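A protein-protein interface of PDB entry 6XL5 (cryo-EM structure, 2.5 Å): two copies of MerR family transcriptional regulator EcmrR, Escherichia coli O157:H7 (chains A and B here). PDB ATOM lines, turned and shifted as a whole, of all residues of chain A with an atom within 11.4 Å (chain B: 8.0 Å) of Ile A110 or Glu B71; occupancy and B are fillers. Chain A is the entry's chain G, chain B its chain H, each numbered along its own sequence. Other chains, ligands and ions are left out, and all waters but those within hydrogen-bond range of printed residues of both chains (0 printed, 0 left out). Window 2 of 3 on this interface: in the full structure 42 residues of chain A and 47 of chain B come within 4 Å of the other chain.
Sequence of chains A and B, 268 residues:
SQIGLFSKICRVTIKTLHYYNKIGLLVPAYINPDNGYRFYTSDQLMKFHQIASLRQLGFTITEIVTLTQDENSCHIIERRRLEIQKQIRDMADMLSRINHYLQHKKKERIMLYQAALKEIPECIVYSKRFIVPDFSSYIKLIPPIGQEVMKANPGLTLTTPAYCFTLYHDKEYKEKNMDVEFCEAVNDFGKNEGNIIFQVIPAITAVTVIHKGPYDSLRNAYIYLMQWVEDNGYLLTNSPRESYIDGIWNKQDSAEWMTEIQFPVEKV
NH2 of Arg A109 is in hydrogen-bond range of SG of Cys B74.
OH of Tyr A101 sits close to NZ of Lys A105, 3.4 Å away.
The side-chain amide oxygen of Gln A114 sits close to the backbone carbonyl oxygen of Met A111.
The backbone carbonyl oxygen (O) of Asn B72 is in hydrogen-bond range of the side-chain sulfur (SG) of Cys B74, 3.4 Å away.
Among the printed residues, pairs that only touch across the chains: Gln A114 with Gln B50 (3.3 Å), Met A111 with Glu B71 (3.8 Å), Tyr A101 with Ile B77 (3.8 Å), Ile A110 with Glu B71 (3.9 Å) and Lys A105 with Cys B74 (3.997 Å).
Ile A110 touches one residue of chain B.
Glu B71 touches two residues of chain A.
No residue of chain A comes within 4 Å of Asp B70.
No residue of chain A comes within 4 Å of Asn B72.
No residue of chain A comes within 4 Å of Ser B73.
Of the printed residues of chain A, Cys B74 touches Lys A105 (3.997 Å) and Arg A109 (3.1 Å).
Of the printed residues of chain B, Tyr A101 touches Ile B77.
Of the printed residues of chain A, Gln B50 touches Gln A114.
Of the printed residues of chain B, Lys A105 touches Cys B74 (3.997 Å).
Leu A112 touches none of the printed residues of chain B.
The nearest printed residue of chain B that does not touch Tyr A101 is Leu B67 (4.6 Å).
Hydrophobic or aromatic side chains of chain B within 4 Å of the printed part of chain A: Ile B77.
Hydrophobic or aromatic side chains of chain A that line the printed part of chain B: Tyr A101 and Ile A110.
Among the printed residues, no Asp or Glu carboxylate lies within 4 Å of a Lys or Arg side-chain nitrogen of the other chain.
No position is printed for both chains.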
ATOM      1  N   HIS A 100      31.778  29.523   1.161  1.00  0.00           N
ATOM      2  CA  HIS A 100      32.264  28.249   1.676  1.00  0.00           C
ATOM      3  C   HIS A 100      31.873  27.111   0.751  1.00  0.00           C
ATOM      4  O   HIS A 100      32.679  26.213   0.471  1.00  0.00           O
ATOM      5  CB  HIS A 100      31.680  28.057   3.078  1.00  0.00           C
ATOM      6  CG  HIS A 100      31.942  26.722   3.697  1.00  0.00           C
ATOM      7  ND1 HIS A 100      32.943  26.523   4.623  1.00  0.00           N
ATOM      8  CD2 HIS A 100      31.292  25.540   3.585  1.00  0.00           C
ATOM      9  CE1 HIS A 100      32.920  25.267   5.029  1.00  0.00           C
ATOM     10  NE2 HIS A 100      31.923  24.650   4.418  1.00  0.00           N
ATOM     11  N   TYR A 101      30.638  27.142   0.259  1.00  0.00           N
ATOM     12  CA  TYR A 101      30.170  26.129  -0.682  1.00  0.00           C
ATOM     13  C   TYR A 101      31.016  26.115  -1.954  1.00  0.00           C
ATOM     14  O   TYR A 101      31.398  25.044  -2.437  1.00  0.00           O
ATOM     15  CB  TYR A 101      28.722  26.410  -1.020  1.00  0.00           C
ATOM     16  CG  TYR A 101      28.010  25.353  -1.840  1.00  0.00           C
ATOM     17  CD1 TYR A 101      28.025  24.028  -1.443  1.00  0.00           C
ATOM     18  CD2 TYR A 101      27.310  25.682  -2.998  1.00  0.00           C
ATOM     19  CE1 TYR A 101      27.373  23.058  -2.172  1.00  0.00           C
ATOM     20  CE2 TYR A 101      26.659  24.712  -3.737  1.00  0.00           C
ATOM     21  CZ  TYR A 101      26.698  23.401  -3.318  1.00  0.00           C
ATOM     22  OH  TYR A 101      26.051  22.424  -4.041  1.00  0.00           O
ATOM     23  N   LEU A 102      31.346  27.288  -2.506  1.00  0.00           N
ATOM     24  CA  LEU A 102      32.221  27.279  -3.682  1.00  0.00           C
ATOM     25  C   LEU A 102      33.653  26.819  -3.351  1.00  0.00           C
ATOM     26  O   LEU A 102      34.243  26.090  -4.152  1.00  0.00           O
ATOM     27  CB  LEU A 102      32.261  28.670  -4.320  1.00  0.00           C
ATOM     28  CG  LEU A 102      33.193  28.838  -5.523  1.00  0.00           C
ATOM     29  CD1 LEU A 102      32.750  27.947  -6.673  1.00  0.00           C
ATOM     30  CD2 LEU A 102      33.252  30.294  -5.958  1.00  0.00           C
ATOM     31  N   GLN A 103      34.262  27.269  -2.240  1.00  0.00           N
ATOM     32  CA  GLN A 103      35.617  26.771  -1.891  1.00  0.00           C
ATOM     33  C   GLN A 103      35.642  25.248  -1.711  1.00  0.00           C
ATOM     34  O   GLN A 103      36.606  24.579  -2.105  1.00  0.00           O
ATOM     35  CB  GLN A 103      36.121  27.456  -0.619  1.00  0.00           C
ATOM     36  CG  GLN A 103      36.380  28.945  -0.774  1.00  0.00           C
ATOM     37  CD  GLN A 103      36.807  29.601   0.522  1.00  0.00           C
ATOM     38  OE1 GLN A 103      36.493  29.111   1.607  1.00  0.00           O
ATOM     39  NE2 GLN A 103      37.528  30.713   0.414  1.00  0.00           N
ATOM     40  N   HIS A 104      34.527  24.663  -1.276  1.00  0.00           N
ATOM     41  CA  HIS A 104      34.473  23.208  -1.107  1.00  0.00           C
ATOM     42  C   HIS A 104      34.197  22.518  -2.434  1.00  0.00           C
ATOM     43  O   HIS A 104      34.696  21.408  -2.663  1.00  0.00           O
ATOM     44  CB  HIS A 104      33.437  22.830  -0.063  1.00  0.00           C
ATOM     45  CG  HIS A 104      33.983  22.834   1.322  1.00  0.00           C
ATOM     46  ND1 HIS A 104      34.830  21.853   1.785  1.00  0.00           N
ATOM     47  CD2 HIS A 104      33.871  23.736   2.320  1.00  0.00           C
ATOM     48  CE1 HIS A 104      35.173  22.125   3.030  1.00  0.00           C
ATOM     49  NE2 HIS A 104      34.608  23.265   3.378  1.00  0.00           N
ATOM     50  N   LYS A 105      33.393  23.117  -3.303  1.00  0.00           N
ATOM     51  CA  LYS A 105      33.087  22.437  -4.550  1.00  0.00           C
ATOM     52  C   LYS A 105      34.350  22.472  -5.399  1.00  0.00           C
ATOM     53  O   LYS A 105      34.673  21.506  -6.098  1.00  0.00           O
ATOM     54  CB  LYS A 105      31.920  23.117  -5.263  1.00  0.00           C
ATOM     55  CG  LYS A 105      31.400  22.368  -6.477  1.00  0.00           C
ATOM     56  CD  LYS A 105      30.038  22.898  -6.884  1.00  0.00           C
ATOM     57  CE  LYS A 105      28.975  22.546  -5.855  1.00  0.00           C
ATOM     58  NZ  LYS A 105      28.696  21.089  -5.808  1.00  0.00           N
ATOM     59  N   LYS A 106      35.054  23.609  -5.376  1.00  0.00           N
ATOM     60  CA  LYS A 106      36.359  23.767  -5.997  1.00  0.00           C
ATOM     61  C   LYS A 106      37.445  22.969  -5.268  1.00  0.00           C
ATOM     62  O   LYS A 106      38.527  22.763  -5.829  1.00  0.00           O
ATOM     63  CB  LYS A 106      36.714  25.258  -5.976  1.00  0.00           C
ATOM     64  CG  LYS A 106      37.993  25.682  -6.667  1.00  0.00           C
ATOM     65  CD  LYS A 106      38.143  27.181  -6.543  1.00  0.00           C
ATOM     66  CE  LYS A 106      38.446  27.547  -5.098  1.00  0.00           C
ATOM     67  NZ  LYS A 106      37.820  28.829  -4.690  1.00  0.00           N
ATOM     68  N   LYS A 107      37.161  22.463  -4.062  1.00  0.00           N
ATOM     69  CA  LYS A 107      38.090  21.608  -3.332  1.00  0.00           C
ATOM     70  C   LYS A 107      37.956  20.146  -3.737  1.00  0.00           C
ATOM     71  O   LYS A 107      38.964  19.486  -4.020  1.00  0.00           O
ATOM     72  CB  LYS A 107      37.830  21.752  -1.826  1.00  0.00           C
ATOM     73  CG  LYS A 107      38.653  20.855  -0.914  1.00  0.00           C
ATOM     74  CD  LYS A 107      38.683  21.411   0.500  1.00  0.00           C
ATOM     75  CE  LYS A 107      39.783  20.794   1.345  1.00  0.00           C
ATOM     76  NZ  LYS A 107      39.864  21.455   2.674  1.00  0.00           N
ATOM     77  N   GLU A 108      36.736  19.612  -3.728  1.00  0.00           N
ATOM     78  CA  GLU A 108      36.520  18.220  -4.089  1.00  0.00           C
ATOM     79  C   GLU A 108      35.459  18.175  -5.193  1.00  0.00           C
ATOM     80  O   GLU A 108      34.475  18.931  -5.159  1.00  0.00           O
ATOM     81  CB  GLU A 108      36.086  17.393  -2.878  1.00  0.00           C
ATOM     82  CG  GLU A 108      37.171  17.213  -1.827  1.00  0.00           C
ATOM     83  CD  GLU A 108      36.679  16.450  -0.611  1.00  0.00           C
ATOM     84  OE1 GLU A 108      35.457  16.227  -0.500  1.00  0.00           O
ATOM     85  OE2 GLU A 108      37.519  16.074   0.235  1.00  0.00           O
ATOM     86  N   ARG A 109      35.678  17.305  -6.189  1.00  0.00           N
ATOM     87  CA  ARG A 109      34.841  17.399  -7.377  1.00  0.00           C
ATOM     88  C   ARG A 109      33.420  16.979  -7.073  1.00  0.00           C
ATOM     89  O   ARG A 109      32.476  17.543  -7.640  1.00  0.00           O
ATOM     90  CB  ARG A 109      35.439  16.512  -8.473  1.00  0.00           C
ATOM     91  CG  ARG A 109      34.694  16.472  -9.793  1.00  0.00           C
ATOM     92  CD  ARG A 109      34.817  17.783 -10.540  1.00  0.00           C
ATOM     93  NE  ARG A 109      33.734  18.704 -10.225  1.00  0.00           N
ATOM     94  CZ  ARG A 109      33.679  19.961 -10.650  1.00  0.00           C
ATOM     95  NH1 ARG A 109      34.649  20.449 -11.408  1.00  0.00           N
ATOM     96  NH2 ARG A 109      32.648  20.726 -10.320  1.00  0.00           N
ATOM     97  N   ILE A 110      33.244  16.015  -6.189  1.00  0.00           N
ATOM     98  CA  ILE A 110      31.922  15.574  -5.779  1.00  0.00           C
ATOM     99  C   ILE A 110      31.727  16.211  -4.414  1.00  0.00           C
ATOM    100  O   ILE A 110      32.704  16.369  -3.667  1.00  0.00           O
ATOM    101  CB  ILE A 110      31.772  14.038  -5.754  1.00  0.00           C
ATOM    102  CG1 ILE A 110      30.293  13.655  -5.660  1.00  0.00           C
ATOM    103  CG2 ILE A 110      32.551  13.401  -4.611  1.00  0.00           C
ATOM    104  CD1 ILE A 110      29.974  12.310  -6.275  1.00  0.00           C
ATOM    105  N   MET A 111      30.525  16.643  -4.081  1.00  0.00           N
ATOM    106  CA  MET A 111      30.300  17.074  -2.709  1.00  0.00           C
ATOM    107  C   MET A 111      29.648  15.912  -1.971  1.00  0.00           C
ATOM    108  O   MET A 111      28.503  15.544  -2.247  1.00  0.00           O
ATOM    109  CB  MET A 111      29.518  18.378  -2.631  1.00  0.00           C
ATOM    110  CG  MET A 111      30.403  19.525  -3.104  1.00  0.00           C
ATOM    111  SD  MET A 111      30.111  21.074  -2.248  1.00  0.00           S
ATOM    112  CE  MET A 111      30.183  20.526  -0.543  1.00  0.00           C
ATOM    113  N   LEU A 112      30.398  15.352  -1.029  1.00  0.00           N
ATOM    114  CA  LEU A 112      29.964  14.232  -0.205  1.00  0.00           C
ATOM    115  C   LEU A 112      29.117  14.689   0.985  1.00  0.00           C
ATOM    116  O   LEU A 112      28.186  13.979   1.380  1.00  0.00           O
ATOM    117  CB  LEU A 112      31.175  13.439   0.293  1.00  0.00           C
ATOM    118  CG  LEU A 112      30.878  12.270   1.234  1.00  0.00           C
ATOM    119  CD1 LEU A 112      30.044  11.212   0.528  1.00  0.00           C
ATOM    120  CD2 LEU A 112      32.169  11.670   1.771  1.00  0.00           C
ATOM    121  N   TYR A 113      29.476  15.845   1.550  1.00  0.00           N
ATOM    122  CA  TYR A 113      28.815  16.371   2.745  1.00  0.00           C
ATOM    123  C   TYR A 113      28.218  17.782   2.752  1.00  0.00           C
ATOM    124  O   TYR A 113      28.924  18.758   3.007  1.00  0.00           O
ATOM    125  CB  TYR A 113      29.788  16.362   3.932  1.00  0.00           C
ATOM    126  CG  TYR A 113      30.441  15.049   4.281  1.00  0.00           C
ATOM    127  CD1 TYR A 113      29.705  13.993   4.799  1.00  0.00           C
ATOM    128  CD2 TYR A 113      31.812  14.888   4.144  1.00  0.00           C
ATOM    129  CE1 TYR A 113      30.314  12.799   5.138  1.00  0.00           C
ATOM    130  CE2 TYR A 113      32.430  13.702   4.482  1.00  0.00           C
ATOM    131  CZ  TYR A 113      31.677  12.663   4.980  1.00  0.00           C
ATOM    132  OH  TYR A 113      32.300  11.484   5.307  1.00  0.00           O
ATOM    133  N   GLN A 114      26.925  17.885   2.478  1.00  0.00           N
ATOM    134  CA  GLN A 114      26.205  19.140   2.636  1.00  0.00           C
ATOM    135  C   GLN A 114      25.934  19.459   4.104  1.00  0.00           C
ATOM    136  O   GLN A 114      25.727  18.566   4.927  1.00  0.00           O
ATOM    137  CB  GLN A 114      24.901  19.053   1.854  1.00  0.00           C
ATOM    138  CG  GLN A 114      25.120  19.088   0.354  1.00  0.00           C
ATOM    139  CD  GLN A 114      25.345  17.709  -0.240  1.00  0.00           C
ATOM    140  OE1 GLN A 114      26.318  17.489  -0.960  1.00  0.00           O
ATOM    141  NE2 GLN A 114      24.487  16.762   0.108  1.00  0.00           N
ATOM    142  N   LYS A 212      26.465   9.103   5.646  1.00  0.00           N
ATOM    143  CA  LYS A 212      26.038   7.779   5.225  1.00  0.00           C
ATOM    144  C   LYS A 212      27.290   6.942   4.997  1.00  0.00           C
ATOM    145  O   LYS A 212      28.233   7.391   4.335  1.00  0.00           O
ATOM    146  CB  LYS A 212      25.130   7.814   3.987  1.00  0.00           C
ATOM    147  CG  LYS A 212      25.757   8.124   2.638  1.00  0.00           C
ATOM    148  CD  LYS A 212      24.744   7.842   1.532  1.00  0.00           C
ATOM    149  CE  LYS A 212      25.362   7.909   0.145  1.00  0.00           C
ATOM    150  NZ  LYS A 212      26.315   6.794  -0.092  1.00  0.00           N
ATOM    151  N   ASN A 220      36.072  12.876   8.805  1.00  0.00           N
ATOM    152  CA  ASN A 220      35.926  13.788   7.679  1.00  0.00           C
ATOM    153  C   ASN A 220      34.812  14.788   7.927  1.00  0.00           C
ATOM    154  O   ASN A 220      35.064  16.001   7.984  1.00  0.00           O
ATOM    155  CB  ASN A 220      35.648  12.990   6.405  1.00  0.00           C
ATOM    156  CG  ASN A 220      36.882  12.320   5.868  1.00  0.00           C
ATOM    157  OD1 ASN A 220      37.808  12.982   5.402  1.00  0.00           O
ATOM    158  ND2 ASN A 220      36.906  10.994   5.926  1.00  0.00           N
ATOM    159  N   TYR A 224      34.991  18.713   8.552  1.00  0.00           N
ATOM    160  CA  TYR A 224      34.208  19.563   7.672  1.00  0.00           C
ATOM    161  C   TYR A 224      33.295  20.471   8.474  1.00  0.00           C
ATOM    162  O   TYR A 224      33.281  21.690   8.249  1.00  0.00           O
ATOM    163  CB  TYR A 224      33.401  18.691   6.713  1.00  0.00           C
ATOM    164  CG  TYR A 224      32.392  19.439   5.877  1.00  0.00           C
ATOM    165  CD1 TYR A 224      32.799  20.229   4.812  1.00  0.00           C
ATOM    166  CD2 TYR A 224      31.028  19.326   6.130  1.00  0.00           C
ATOM    167  CE1 TYR A 224      31.885  20.900   4.029  1.00  0.00           C
ATOM    168  CE2 TYR A 224      30.103  19.997   5.349  1.00  0.00           C
ATOM    169  CZ  TYR A 224      30.538  20.781   4.302  1.00  0.00           C
ATOM    170  OH  TYR A 224      29.624  21.450   3.523  1.00  0.00           O
ATOM    171  N   GLN B  50      20.053  17.874   1.693  1.00  0.00           N
ATOM    172  CA  GLN B  50      20.727  18.761   0.768  1.00  0.00           C
ATOM    173  C   GLN B  50      19.763  19.740   0.112  1.00  0.00           C
ATOM    174  O   GLN B  50      20.164  20.867  -0.214  1.00  0.00           O
ATOM    175  CB  GLN B  50      21.465  17.910  -0.257  1.00  0.00           C
ATOM    176  CG  GLN B  50      20.542  17.233  -1.190  1.00  0.00           C
ATOM    177  CD  GLN B  50      20.314  17.971  -2.455  1.00  0.00           C
ATOM    178  OE1 GLN B  50      20.787  19.108  -2.625  1.00  0.00           O
ATOM    179  NE2 GLN B  50      19.574  17.359  -3.356  1.00  0.00           N
ATOM    180  N   THR B  66      17.542  21.901 -10.886  1.00  0.00           N
ATOM    181  CA  THR B  66      18.640  21.691 -11.824  1.00  0.00           C
ATOM    182  C   THR B  66      19.950  21.368 -11.107  1.00  0.00           C
ATOM    183  O   THR B  66      20.710  20.500 -11.551  1.00  0.00           O
ATOM    184  CB  THR B  66      18.814  22.867 -12.807  1.00  0.00           C
ATOM    185  OG1 THR B  66      19.818  22.532 -13.772  1.00  0.00           O
ATOM    186  CG2 THR B  66      19.192  24.166 -12.144  1.00  0.00           C
ATOM    187  N   LEU B  67      20.183  22.031  -9.965  1.00  0.00           N
ATOM    188  CA  LEU B  67      21.394  21.885  -9.161  1.00  0.00           C
ATOM    189  C   LEU B  67      21.572  20.510  -8.532  1.00  0.00           C
ATOM    190  O   LEU B  67      22.715  20.088  -8.327  1.00  0.00           O
ATOM    191  CB  LEU B  67      21.406  22.952  -8.065  1.00  0.00           C
ATOM    192  CG  LEU B  67      22.757  23.376  -7.489  1.00  0.00           C
ATOM    193  CD1 LEU B  67      23.641  23.996  -8.560  1.00  0.00           C
ATOM    194  CD2 LEU B  67      22.567  24.334  -6.328  1.00  0.00           C
ATOM    195  N   THR B  68      20.500  19.790  -8.208  1.00  0.00           N
ATOM    196  CA  THR B  68      20.722  18.546  -7.477  1.00  0.00           C
ATOM    197  C   THR B  68      20.771  17.299  -8.345  1.00  0.00           C
ATOM    198  O   THR B  68      21.074  16.221  -7.825  1.00  0.00           O
ATOM    199  CB  THR B  68      19.642  18.359  -6.418  1.00  0.00           C
ATOM    200  OG1 THR B  68      18.394  18.052  -7.047  1.00  0.00           O
ATOM    201  CG2 THR B  68      19.503  19.615  -5.622  1.00  0.00           C
ATOM    202  N   GLN B  69      20.483  17.405  -9.633  1.00  0.00           N
ATOM    203  CA  GLN B  69      20.714  16.299 -10.549  1.00  0.00           C
ATOM    204  C   GLN B  69      21.778  16.609 -11.586  1.00  0.00           C
ATOM    205  O   GLN B  69      22.519  15.701 -11.969  1.00  0.00           O
ATOM    206  CB  GLN B  69      19.418  15.823 -11.227  1.00  0.00           C
ATOM    207  CG  GLN B  69      18.213  15.563 -10.304  1.00  0.00           C
ATOM    208  CD  GLN B  69      17.551  16.806  -9.790  1.00  0.00           C
ATOM    209  OE1 GLN B  69      17.881  17.892 -10.221  1.00  0.00           O
ATOM    210  NE2 GLN B  69      16.612  16.654  -8.865  1.00  0.00           N
ATOM    211  N   ASP B  70      21.900  17.858 -12.044  1.00  0.00           N
ATOM    212  CA  ASP B  70      23.013  18.188 -12.929  1.00  0.00           C
ATOM    213  C   ASP B  70      24.142  18.741 -12.061  1.00  0.00           C
ATOM    214  O   ASP B  70      24.446  19.936 -12.038  1.00  0.00           O
ATOM    215  CB  ASP B  70      22.577  19.174 -14.003  1.00  0.00           C
ATOM    216  CG  ASP B  70      23.621  19.357 -15.092  1.00  0.00           C
ATOM    217  OD1 ASP B  70      23.535  20.355 -15.837  1.00  0.00           O
ATOM    218  OD2 ASP B  70      24.530  18.508 -15.201  1.00  0.00           O
ATOM    219  N   GLU B  71      24.754  17.807 -11.324  1.00  0.00           N
ATOM    220  CA  GLU B  71      25.713  18.122 -10.266  1.00  0.00           C
ATOM    221  C   GLU B  71      26.906  18.926 -10.768  1.00  0.00           C
ATOM    222  O   GLU B  71      27.520  19.668  -9.993  1.00  0.00           O
ATOM    223  CB  GLU B  71      26.164  16.867  -9.525  1.00  0.00           C
ATOM    224  CG  GLU B  71      26.410  17.196  -8.050  1.00  0.00           C
ATOM    225  CD  GLU B  71      26.735  15.995  -7.195  1.00  0.00           C
ATOM    226  OE1 GLU B  71      26.382  14.865  -7.587  1.00  0.00           O
ATOM    227  OE2 GLU B  71      27.327  16.189  -6.113  1.00  0.00           O
ATOM    228  N   ASN B  72      27.252  18.801 -12.051  1.00  0.00           N
ATOM    229  CA  ASN B  72      28.433  19.485 -12.555  1.00  0.00           C
ATOM    230  C   ASN B  72      28.192  20.954 -12.850  1.00  0.00           C
ATOM    231  O   ASN B  72      29.149  21.656 -13.197  1.00  0.00           O
ATOM    232  CB  ASN B  72      28.946  18.771 -13.814  1.00  0.00           C
ATOM    233  CG  ASN B  72      27.947  18.803 -14.973  1.00  0.00           C
ATOM    234  OD1 ASN B  72      27.546  19.864 -15.457  1.00  0.00           O
ATOM    235  ND2 ASN B  72      27.543  17.617 -15.423  1.00  0.00           N
ATOM    236  N   SER B  73      26.952  21.427 -12.764  1.00  0.00           N
ATOM    237  CA  SER B  73      26.669  22.820 -13.074  1.00  0.00           C
ATOM    238  C   SER B  73      27.330  23.609 -11.954  1.00  0.00           C
ATOM    239  O   SER B  73      26.935  23.493 -10.789  1.00  0.00           O
ATOM    240  CB  SER B  73      25.170  23.081 -13.150  1.00  0.00           C
ATOM    241  OG  SER B  73      24.912  24.440 -13.453  1.00  0.00           O
ATOM    242  N   CYS B  74      28.337  24.406 -12.295  1.00  0.00           N
ATOM    243  CA  CYS B  74      29.033  25.219 -11.312  1.00  0.00           C
ATOM    244  C   CYS B  74      28.883  26.713 -11.488  1.00  0.00           C
ATOM    245  O   CYS B  74      29.084  27.438 -10.512  1.00  0.00           O
ATOM    246  CB  CYS B  74      30.533  24.884 -11.316  1.00  0.00           C
ATOM    247  SG  CYS B  74      30.910  23.206 -10.773  1.00  0.00           S
ATOM    248  N   ILE B  77      26.571  28.803  -9.004  1.00  0.00           N
ATOM    249  CA  ILE B  77      26.914  29.195  -7.641  1.00  0.00           C
ATOM    250  C   ILE B  77      27.633  30.532  -7.628  1.00  0.00           C
ATOM    251  O   ILE B  77      27.339  31.376  -6.778  1.00  0.00           O
ATOM    252  CB  ILE B  77      27.725  28.090  -6.942  1.00  0.00           C
ATOM    253  CG1 ILE B  77      26.995  26.744  -7.052  1.00  0.00           C
ATOM    254  CG2 ILE B  77      28.035  28.473  -5.508  1.00  0.00           C
ATOM    255  CD1 ILE B  77      27.546  25.792  -8.078  1.00  0.00           C
